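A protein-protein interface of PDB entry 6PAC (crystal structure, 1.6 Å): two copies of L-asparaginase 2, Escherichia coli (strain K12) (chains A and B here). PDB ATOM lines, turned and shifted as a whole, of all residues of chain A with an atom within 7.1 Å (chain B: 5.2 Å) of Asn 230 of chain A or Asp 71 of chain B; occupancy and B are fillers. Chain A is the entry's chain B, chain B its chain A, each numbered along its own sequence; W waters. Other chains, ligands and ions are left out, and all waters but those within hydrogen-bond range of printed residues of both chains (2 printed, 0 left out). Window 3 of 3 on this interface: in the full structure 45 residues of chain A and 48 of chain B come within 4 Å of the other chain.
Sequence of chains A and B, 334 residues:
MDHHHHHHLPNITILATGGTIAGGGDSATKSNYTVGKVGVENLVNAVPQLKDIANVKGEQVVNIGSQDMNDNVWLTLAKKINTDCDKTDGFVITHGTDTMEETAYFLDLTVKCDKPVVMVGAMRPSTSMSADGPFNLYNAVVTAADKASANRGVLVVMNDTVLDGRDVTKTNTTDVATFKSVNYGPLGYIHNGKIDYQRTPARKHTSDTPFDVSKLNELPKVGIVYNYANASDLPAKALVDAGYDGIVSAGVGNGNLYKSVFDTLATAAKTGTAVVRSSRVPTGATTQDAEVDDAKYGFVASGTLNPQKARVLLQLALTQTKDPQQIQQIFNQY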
ATOM      1  N   TYR A 228      -7.097 -11.046  14.493  1.00  0.00           N
ATOM      2  CA  TYR A 228      -7.318  -9.857  13.656  1.00  0.00           C
ATOM      3  C   TYR A 228      -6.401 -10.143  12.448  1.00  0.00           C
ATOM      4  O   TYR A 228      -5.648 -11.144  12.449  1.00  0.00           O
ATOM      5  CB  TYR A 228      -6.992  -8.526  14.391  1.00  0.00           C
ATOM      6  CG  TYR A 228      -5.610  -8.540  14.993  1.00  0.00           C
ATOM      7  CD1 TYR A 228      -5.408  -9.164  16.220  1.00  0.00           C
ATOM      8  CD2 TYR A 228      -4.562  -8.004  14.329  1.00  0.00           C
ATOM      9  CE1 TYR A 228      -4.141  -9.180  16.807  1.00  0.00           C
ATOM     10  CE2 TYR A 228      -3.276  -8.003  14.888  1.00  0.00           C
ATOM     11  CZ  TYR A 228      -3.093  -8.592  16.121  1.00  0.00           C
ATOM     12  OH  TYR A 228      -1.786  -8.599  16.559  1.00  0.00           O
ATOM     13  N   ALA A 229      -6.492  -9.314  11.432  1.00  0.00           N
ATOM     14  CA  ALA A 229      -5.676  -9.479  10.238  1.00  0.00           C
ATOM     15  C   ALA A 229      -4.189  -9.321  10.614  1.00  0.00           C
ATOM     16  O   ALA A 229      -3.806  -8.482  11.452  1.00  0.00           O
ATOM     17  CB  ALA A 229      -6.060  -8.448   9.189  1.00  0.00           C
ATOM     18  N   ASN A 230      -3.358 -10.209  10.065  1.00  0.00           N
ATOM     19  CA  ASN A 230      -1.923 -10.171  10.352  1.00  0.00           C
ATOM     20  C   ASN A 230      -1.572 -10.330  11.834  1.00  0.00           C
ATOM     21  O   ASN A 230      -0.532  -9.782  12.327  1.00  0.00           O
ATOM     22  CB  ASN A 230      -1.318  -8.891   9.803  1.00  0.00           C
ATOM     23  CG  ASN A 230       0.083  -9.106   9.183  1.00  0.00           C
ATOM     24  OD1 ASN A 230       0.271  -8.927   7.969  1.00  0.00           O
ATOM     25  ND2 ASN A 230       1.067  -9.513  10.035  1.00  0.00           N
ATOM     26  N   ALA A 231      -2.381 -11.077  12.572  1.00  0.00           N
ATOM     27  CA  ALA A 231      -2.125 -11.216  14.015  1.00  0.00           C
ATOM     28  C   ALA A 231      -0.820 -11.844  14.366  1.00  0.00           C
ATOM     29  O   ALA A 231      -0.410 -12.793  13.715  1.00  0.00           O
ATOM     30  CB  ALA A 231      -3.233 -12.017  14.647  1.00  0.00           C
ATOM     31  N   SER A 232      -0.199 -11.329  15.401  1.00  0.00           N
ATOM     32  CA  SER A 232       1.015 -11.928  15.919  1.00  0.00           C
ATOM     33  C   SER A 232       0.722 -13.184  16.702  1.00  0.00           C
ATOM     34  O   SER A 232      -0.250 -13.249  17.475  1.00  0.00           O
ATOM     35  CB  SER A 232       1.750 -10.936  16.852  1.00  0.00           C
ATOM     36  OG  SER A 232       2.945 -11.547  17.328  1.00  0.00           O
ATOM     37  N   ASP A 233       1.632 -14.151  16.592  1.00  0.00           N
ATOM     38  CA  ASP A 233       1.606 -15.306  17.466  1.00  0.00           C
ATOM     39  C   ASP A 233       2.345 -15.099  18.797  1.00  0.00           C
ATOM     40  O   ASP A 233       2.335 -16.013  19.624  1.00  0.00           O
ATOM     41  CB  ASP A 233       2.127 -16.593  16.769  1.00  0.00           C
ATOM     42  CG  ASP A 233       3.607 -16.509  16.348  1.00  0.00           C
ATOM     43  OD1 ASP A 233       4.297 -15.554  16.733  1.00  0.00           O
ATOM     44  OD2 ASP A 233       4.125 -17.478  15.675  1.00  0.00           O
ATOM     45  N   TYR A 258      -6.241 -16.684  13.050  1.00  0.00           N
ATOM     46  CA  TYR A 258      -5.204 -16.334  12.114  1.00  0.00           C
ATOM     47  C   TYR A 258      -4.184 -17.459  12.052  1.00  0.00           C
ATOM     48  O   TYR A 258      -3.885 -18.077  13.077  1.00  0.00           O
ATOM     49  CB  TYR A 258      -4.525 -14.978  12.527  1.00  0.00           C
ATOM     50  CG  TYR A 258      -3.488 -14.573  11.564  1.00  0.00           C
ATOM     51  CD1 TYR A 258      -3.832 -13.985  10.392  1.00  0.00           C
ATOM     52  CD2 TYR A 258      -2.142 -14.720  11.834  1.00  0.00           C
ATOM     53  CE1 TYR A 258      -2.893 -13.582   9.454  1.00  0.00           C
ATOM     54  CE2 TYR A 258      -1.184 -14.324  10.920  1.00  0.00           C
ATOM     55  CZ  TYR A 258      -1.552 -13.736   9.754  1.00  0.00           C
ATOM     56  OH  TYR A 258      -0.651 -13.300   8.803  1.00  0.00           O
ATOM     57  N   SER A 260      -0.960 -18.082  12.032  1.00  0.00           N
ATOM     58  CA  SER A 260       0.154 -18.242  12.967  1.00  0.00           C
ATOM     59  C   SER A 260      -0.365 -18.567  14.380  1.00  0.00           C
ATOM     60  O   SER A 260       0.250 -19.371  15.056  1.00  0.00           O
ATOM     61  CB  SER A 260       1.080 -17.040  12.946  1.00  0.00           C
ATOM     62  OG  SER A 260       0.486 -15.917  13.500  1.00  0.00           O
ATOM     63  N   MET B  69      -6.276 -12.902   6.409  1.00  0.00           N
ATOM     64  CA  MET B  69      -6.009 -11.612   5.783  1.00  0.00           C
ATOM     65  C   MET B  69      -4.771 -11.013   6.449  1.00  0.00           C
ATOM     66  O   MET B  69      -4.465 -11.277   7.627  1.00  0.00           O
ATOM     67  CB  MET B  69      -7.254 -10.750   5.940  1.00  0.00           C
ATOM     68  CG  MET B  69      -7.218  -9.421   5.251  1.00  0.00           C
ATOM     69  SD  MET B  69      -6.882  -9.525   3.470  1.00  0.00           S
ATOM     70  CE  MET B  69      -8.079 -10.683   2.914  1.00  0.00           C
ATOM     71  N   ASN B  70      -4.056 -10.236   5.684  1.00  0.00           N
ATOM     72  CA  ASN B  70      -2.776  -9.678   6.138  1.00  0.00           C
ATOM     73  C   ASN B  70      -2.395  -8.402   5.392  1.00  0.00           C
ATOM     74  O   ASN B  70      -3.083  -7.965   4.453  1.00  0.00           O
ATOM     75  CB  ASN B  70      -1.693 -10.778   6.003  1.00  0.00           C
ATOM     76  CG  ASN B  70      -1.456 -11.126   4.535  1.00  0.00           C
ATOM     77  OD1 ASN B  70      -1.105 -10.277   3.742  1.00  0.00           O
ATOM     78  ND2 ASN B  70      -1.831 -12.354   4.141  1.00  0.00           N
ATOM     79  N   ASP B  71      -1.351  -7.750   5.906  1.00  0.00           N
ATOM     80  CA  ASP B  71      -0.918  -6.435   5.437  1.00  0.00           C
ATOM     81  C   ASP B  71      -0.608  -6.506   3.910  1.00  0.00           C
ATOM     82  O   ASP B  71      -0.810  -5.556   3.188  1.00  0.00           O
ATOM     83  CB  ASP B  71       0.381  -5.935   6.129  1.00  0.00           C
ATOM     84  CG  ASP B  71       0.232  -5.630   7.640  1.00  0.00           C
ATOM     85  OD1 ASP B  71      -0.920  -5.690   8.146  1.00  0.00           O
ATOM     86  OD2 ASP B  71       1.301  -5.425   8.257  1.00  0.00           O
ATOM     87  N   ASN B  72      -0.035  -7.604   3.452  1.00  0.00           N
ATOM     88  CA  ASN B  72       0.373  -7.643   2.053  1.00  0.00           C
ATOM     89  C   ASN B  72      -0.807  -7.636   1.096  1.00  0.00           C
ATOM     90  O   ASN B  72      -0.762  -7.003   0.024  1.00  0.00           O
ATOM     91  CB  ASN B  72       1.279  -8.819   1.751  1.00  0.00           C
ATOM     92  CG  ASN B  72       2.041  -8.562   0.464  1.00  0.00           C
ATOM     93  OD1 ASN B  72       2.757  -7.569   0.410  1.00  0.00           O
ATOM     94  ND2 ASN B  72       1.772  -9.346  -0.634  1.00  0.00           N
ATOM     95  N   VAL B  73      -1.888  -8.297   1.480  1.00  0.00           N
ATOM     96  CA  VAL B  73      -3.092  -8.318   0.651  1.00  0.00           C
ATOM     97  C   VAL B  73      -3.681  -6.906   0.661  1.00  0.00           C
ATOM     98  O   VAL B  73      -4.171  -6.429  -0.356  1.00  0.00           O
ATOM     99  CB  VAL B  73      -4.090  -9.375   1.062  1.00  0.00           C
ATOM    100  CG1 VAL B  73      -5.398  -9.248   0.265  1.00  0.00           C
ATOM    101  CG2 VAL B  73      -3.460 -10.754   0.921  1.00  0.00           C
ATOM    102  N   TRP B  74      -3.673  -6.258   1.825  1.00  0.00           N
ATOM    103  CA  TRP B  74      -4.145  -4.857   1.905  1.00  0.00           C
ATOM    104  C   TRP B  74      -3.401  -3.947   0.985  1.00  0.00           C
ATOM    105  O   TRP B  74      -4.013  -3.169   0.232  1.00  0.00           O
ATOM    106  CB  TRP B  74      -3.988  -4.347   3.341  1.00  0.00           C
ATOM    107  CG  TRP B  74      -5.050  -4.903   4.290  1.00  0.00           C
ATOM    108  CD1 TRP B  74      -6.038  -5.793   3.999  1.00  0.00           C
ATOM    109  CD2 TRP B  74      -5.126  -4.650   5.693  1.00  0.00           C
ATOM    110  NE1 TRP B  74      -6.780  -6.060   5.110  1.00  0.00           N
ATOM    111  CE2 TRP B  74      -6.246  -5.357   6.174  1.00  0.00           C
ATOM    112  CE3 TRP B  74      -4.402  -3.819   6.593  1.00  0.00           C
ATOM    113  CZ2 TRP B  74      -6.607  -5.328   7.492  1.00  0.00           C
ATOM    114  CZ3 TRP B  74      -4.787  -3.780   7.900  1.00  0.00           C
ATOM    115  CH2 TRP B  74      -5.891  -4.559   8.340  1.00  0.00           C
ATOM    116  N   LEU B  75      -2.066  -4.017   1.058  1.00  0.00           N
ATOM    117  CA  LEU B  75      -1.258  -3.183   0.120  1.00  0.00           C
ATOM    118  C   LEU B  75      -1.527  -3.515  -1.358  1.00  0.00           C
ATOM    119  O   LEU B  75      -1.647  -2.592  -2.195  1.00  0.00           O
ATOM    120  CB  LEU B  75       0.228  -3.323   0.429  1.00  0.00           C
ATOM    121  CG  LEU B  75       0.646  -2.653   1.742  1.00  0.00           C
ATOM    122  CD1 LEU B  75       2.035  -3.010   2.172  1.00  0.00           C
ATOM    123  CD2 LEU B  75       0.528  -1.120   1.620  1.00  0.00           C
ATOM    124  N   THR B  76      -1.644  -4.809  -1.653  1.00  0.00           N
ATOM    125  CA  THR B  76      -1.957  -5.242  -3.027  1.00  0.00           C
ATOM    126  C   THR B  76      -3.268  -4.647  -3.514  1.00  0.00           C
ATOM    127  O   THR B  76      -3.364  -4.142  -4.643  1.00  0.00           O
ATOM    128  CB  THR B  76      -2.051  -6.753  -3.072  1.00  0.00           C
ATOM    129  OG1 THR B  76      -0.796  -7.314  -2.707  1.00  0.00           O
ATOM    130  CG2 THR B  76      -2.488  -7.307  -4.472  1.00  0.00           C
ATOM    131  N   LEU B 219       3.758  -2.548   6.422  1.00  0.00           N
ATOM    132  CA  LEU B 219       3.198  -1.594   7.375  1.00  0.00           C
ATOM    133  C   LEU B 219       3.781  -1.746   8.786  1.00  0.00           C
ATOM    134  O   LEU B 219       4.239  -2.866   9.205  1.00  0.00           O
ATOM    135  CB  LEU B 219       1.675  -1.821   7.445  1.00  0.00           C
ATOM    136  CG  LEU B 219       0.859  -1.729   6.154  1.00  0.00           C
ATOM    137  CD1 LEU B 219      -0.573  -2.302   6.359  1.00  0.00           C
ATOM    138  CD2 LEU B 219       0.783  -0.317   5.660  1.00  0.00           C
ATOM    139  N   PRO B 220       3.718  -0.665   9.562  1.00  0.00           N
ATOM    140  CA  PRO B 220       4.197  -0.756  10.930  1.00  0.00           C
ATOM    141  C   PRO B 220       3.549  -1.889  11.743  1.00  0.00           C
ATOM    142  O   PRO B 220       2.421  -2.290  11.505  1.00  0.00           O
ATOM    143  CB  PRO B 220       3.889   0.597  11.508  1.00  0.00           C
ATOM    144  CG  PRO B 220       3.848   1.499  10.332  1.00  0.00           C
ATOM    145  CD  PRO B 220       3.244   0.686   9.236  1.00  0.00           C
ATOM    146  N   ARG B 311      -6.253  -0.618  15.292  1.00  0.00           N
ATOM    147  CA  ARG B 311      -5.018  -1.109  14.680  1.00  0.00           C
ATOM    148  C   ARG B 311      -4.791  -0.563  13.283  1.00  0.00           C
ATOM    149  O   ARG B 311      -3.675  -0.095  12.965  1.00  0.00           O
ATOM    150  CB  ARG B 311      -4.906  -2.617  14.704  1.00  0.00           C
ATOM    151  CG  ARG B 311      -3.799  -3.181  13.864  1.00  0.00           C
ATOM    152  CD  ARG B 311      -3.604  -4.688  13.998  1.00  0.00           C
ATOM    153  NE  ARG B 311      -2.517  -5.120  13.099  1.00  0.00           N
ATOM    154  CZ  ARG B 311      -2.636  -5.390  11.796  1.00  0.00           C
ATOM    155  NH1 ARG B 311      -3.807  -5.335  11.181  1.00  0.00           N
ATOM    156  NH2 ARG B 311      -1.562  -5.745  11.094  1.00  0.00           N
ATOM    157  N   GLN B 315      -1.556   1.816  12.495  1.00  0.00           N
ATOM    158  CA  GLN B 315      -0.503   1.449  11.541  1.00  0.00           C
ATOM    159  C   GLN B 315      -0.292   2.582  10.548  1.00  0.00           C
ATOM    160  O   GLN B 315       0.842   2.995  10.307  1.00  0.00           O
ATOM    161  CB  GLN B 315      -0.854   0.157  10.727  1.00  0.00           C
ATOM    162  CG  GLN B 315      -0.771  -1.138  11.445  1.00  0.00           C
ATOM    163  CD  GLN B 315      -1.099  -2.254  10.498  1.00  0.00           C
ATOM    164  OE1 GLN B 315      -2.251  -2.347  10.051  1.00  0.00           O
ATOM    165  NE2 GLN B 315      -0.111  -3.086  10.162  1.00  0.00           N
HETATM  166  O   HOH W   1      -1.270 -14.275   6.390  1.00  0.00           O
HETATM  167  O   HOH W   2       1.835  -9.248   5.691  1.00  0.00           O
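N of Asp 71 of chain B lies within hydrogen-bond range of OD1 of Asn 230 of chain A, 2.9 Å away.
The backbone NH (N) of Asn 230 of chain A sits at hydrogen-bond distance from the backbone carbonyl oxygen (O) of Met 69 of chain B (2.9 Å).
The backbone carbonyl oxygen (O) of Ala 229 of chain A sits at hydrogen-bond distance from the guanidinium group (NH1) of Arg 311 of chain B (3.2 Å).
The side-chain carboxylate of Asp 71 of chain B is in salt-bridge range of the guanidinium group of Arg 311 of chain B.
The side-chain amide oxygen (OD1) of Asn 70 of chain B sits at hydrogen-bond distance from the backbone NH (N) of Asn 72 of chain B (2.9 Å).
The side-chain carboxylate of Asp 71 of chain B sits at hydrogen-bond distance from the side-chain amide nitrogen of Gln 315 of chain B (3.3 Å).
The guanidinium group (NH2) of Arg 311 of chain B sits close to the side-chain amide nitrogen (NE2) of Gln 315 of chain B (3.2 Å).
N of Ser 232 of chain A is in hydrogen-bond range of OH of Tyr 228 of chain A.
The side-chain amide oxygen of Asn 70 of chain B sits at hydrogen-bond distance from the backbone NH of Val 73 of chain B, at 3.1 Å.
Among the printed residues, pairs that only touch across the chains: Tyr 258 of chain A with Met 69 of chain B (3.3 Å), Asn 230 of chain A with Asn 70 of chain B (3.3 Å), Ala 229 of chain A with Met 69 of chain B (3.4 Å), Asn 230 of chain A with Arg 311 of chain B (3.4 Å), Tyr 228 of chain A with Arg 311 of chain B (3.4 Å), Ala 229 of chain A with Trp 74 of chain B (3.6 Å) and Tyr 258 of chain A with Asn 70 of chain B (3.9 Å).
Of chain B, only Met 69 (2.9 Å), Asn 70 (3.3 Å), Asp 71 (2.9 Å) and Arg 311 (3.4 Å) come within 4 Å of Asn 230 of chain A.
Asp 71 of chain B touches one residue of chain A.
Of the printed residues of chain A, Trp 74 of chain B touches Ala 229.
Of the printed residues of chain B, Tyr 258 of chain A touches Met 69 (3.3 Å) and Asn 70 (3.9 Å).
Printed residues of chain A within 4 Å of Met 69 of chain B: Ala 229, Asn 230 and Tyr 258.
Printed residues of chain B within 4 Å of Tyr 228 of chain A: Arg 311.
Of the printed residues of chain A, Asn 70 of chain B touches Asn 230 and Tyr 258.
Leu 219 of chain B touches none of the printed residues of chain A.
Thr 76 of chain B touches none of the printed residues of chain A.
The nearest printed residue of chain B that does not touch Ala 229 of chain A is Asn 70 of chain B (4.4 Å).
Of the 12 printed residues of chain B, 5 touch a printed residue of chain A.
Hydrophobic or aromatic side chains of chain B that line the printed part of chain A: Trp 74.
Among the printed residues, 10 pairs touch across the chains.
Among the printed residues, no Asp or Glu carboxylate lies within 4 Å of a Lys or Arg side-chain nitrogen of the other chain.
No position is printed for both chains.
Of the 10 pairs that touch across the chains among the printed residues, none has its exchanged pair printed and touching as well.
Water W1 bridges OH of Tyr 258 of chain A (2.7 Å) and ND2 of Asn 70 of chain B (3.0 Å).
Water W2 lies within hydrogen-bond range of OD1 of Asn 230 of chain A and N of Asn 72 of chain B.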
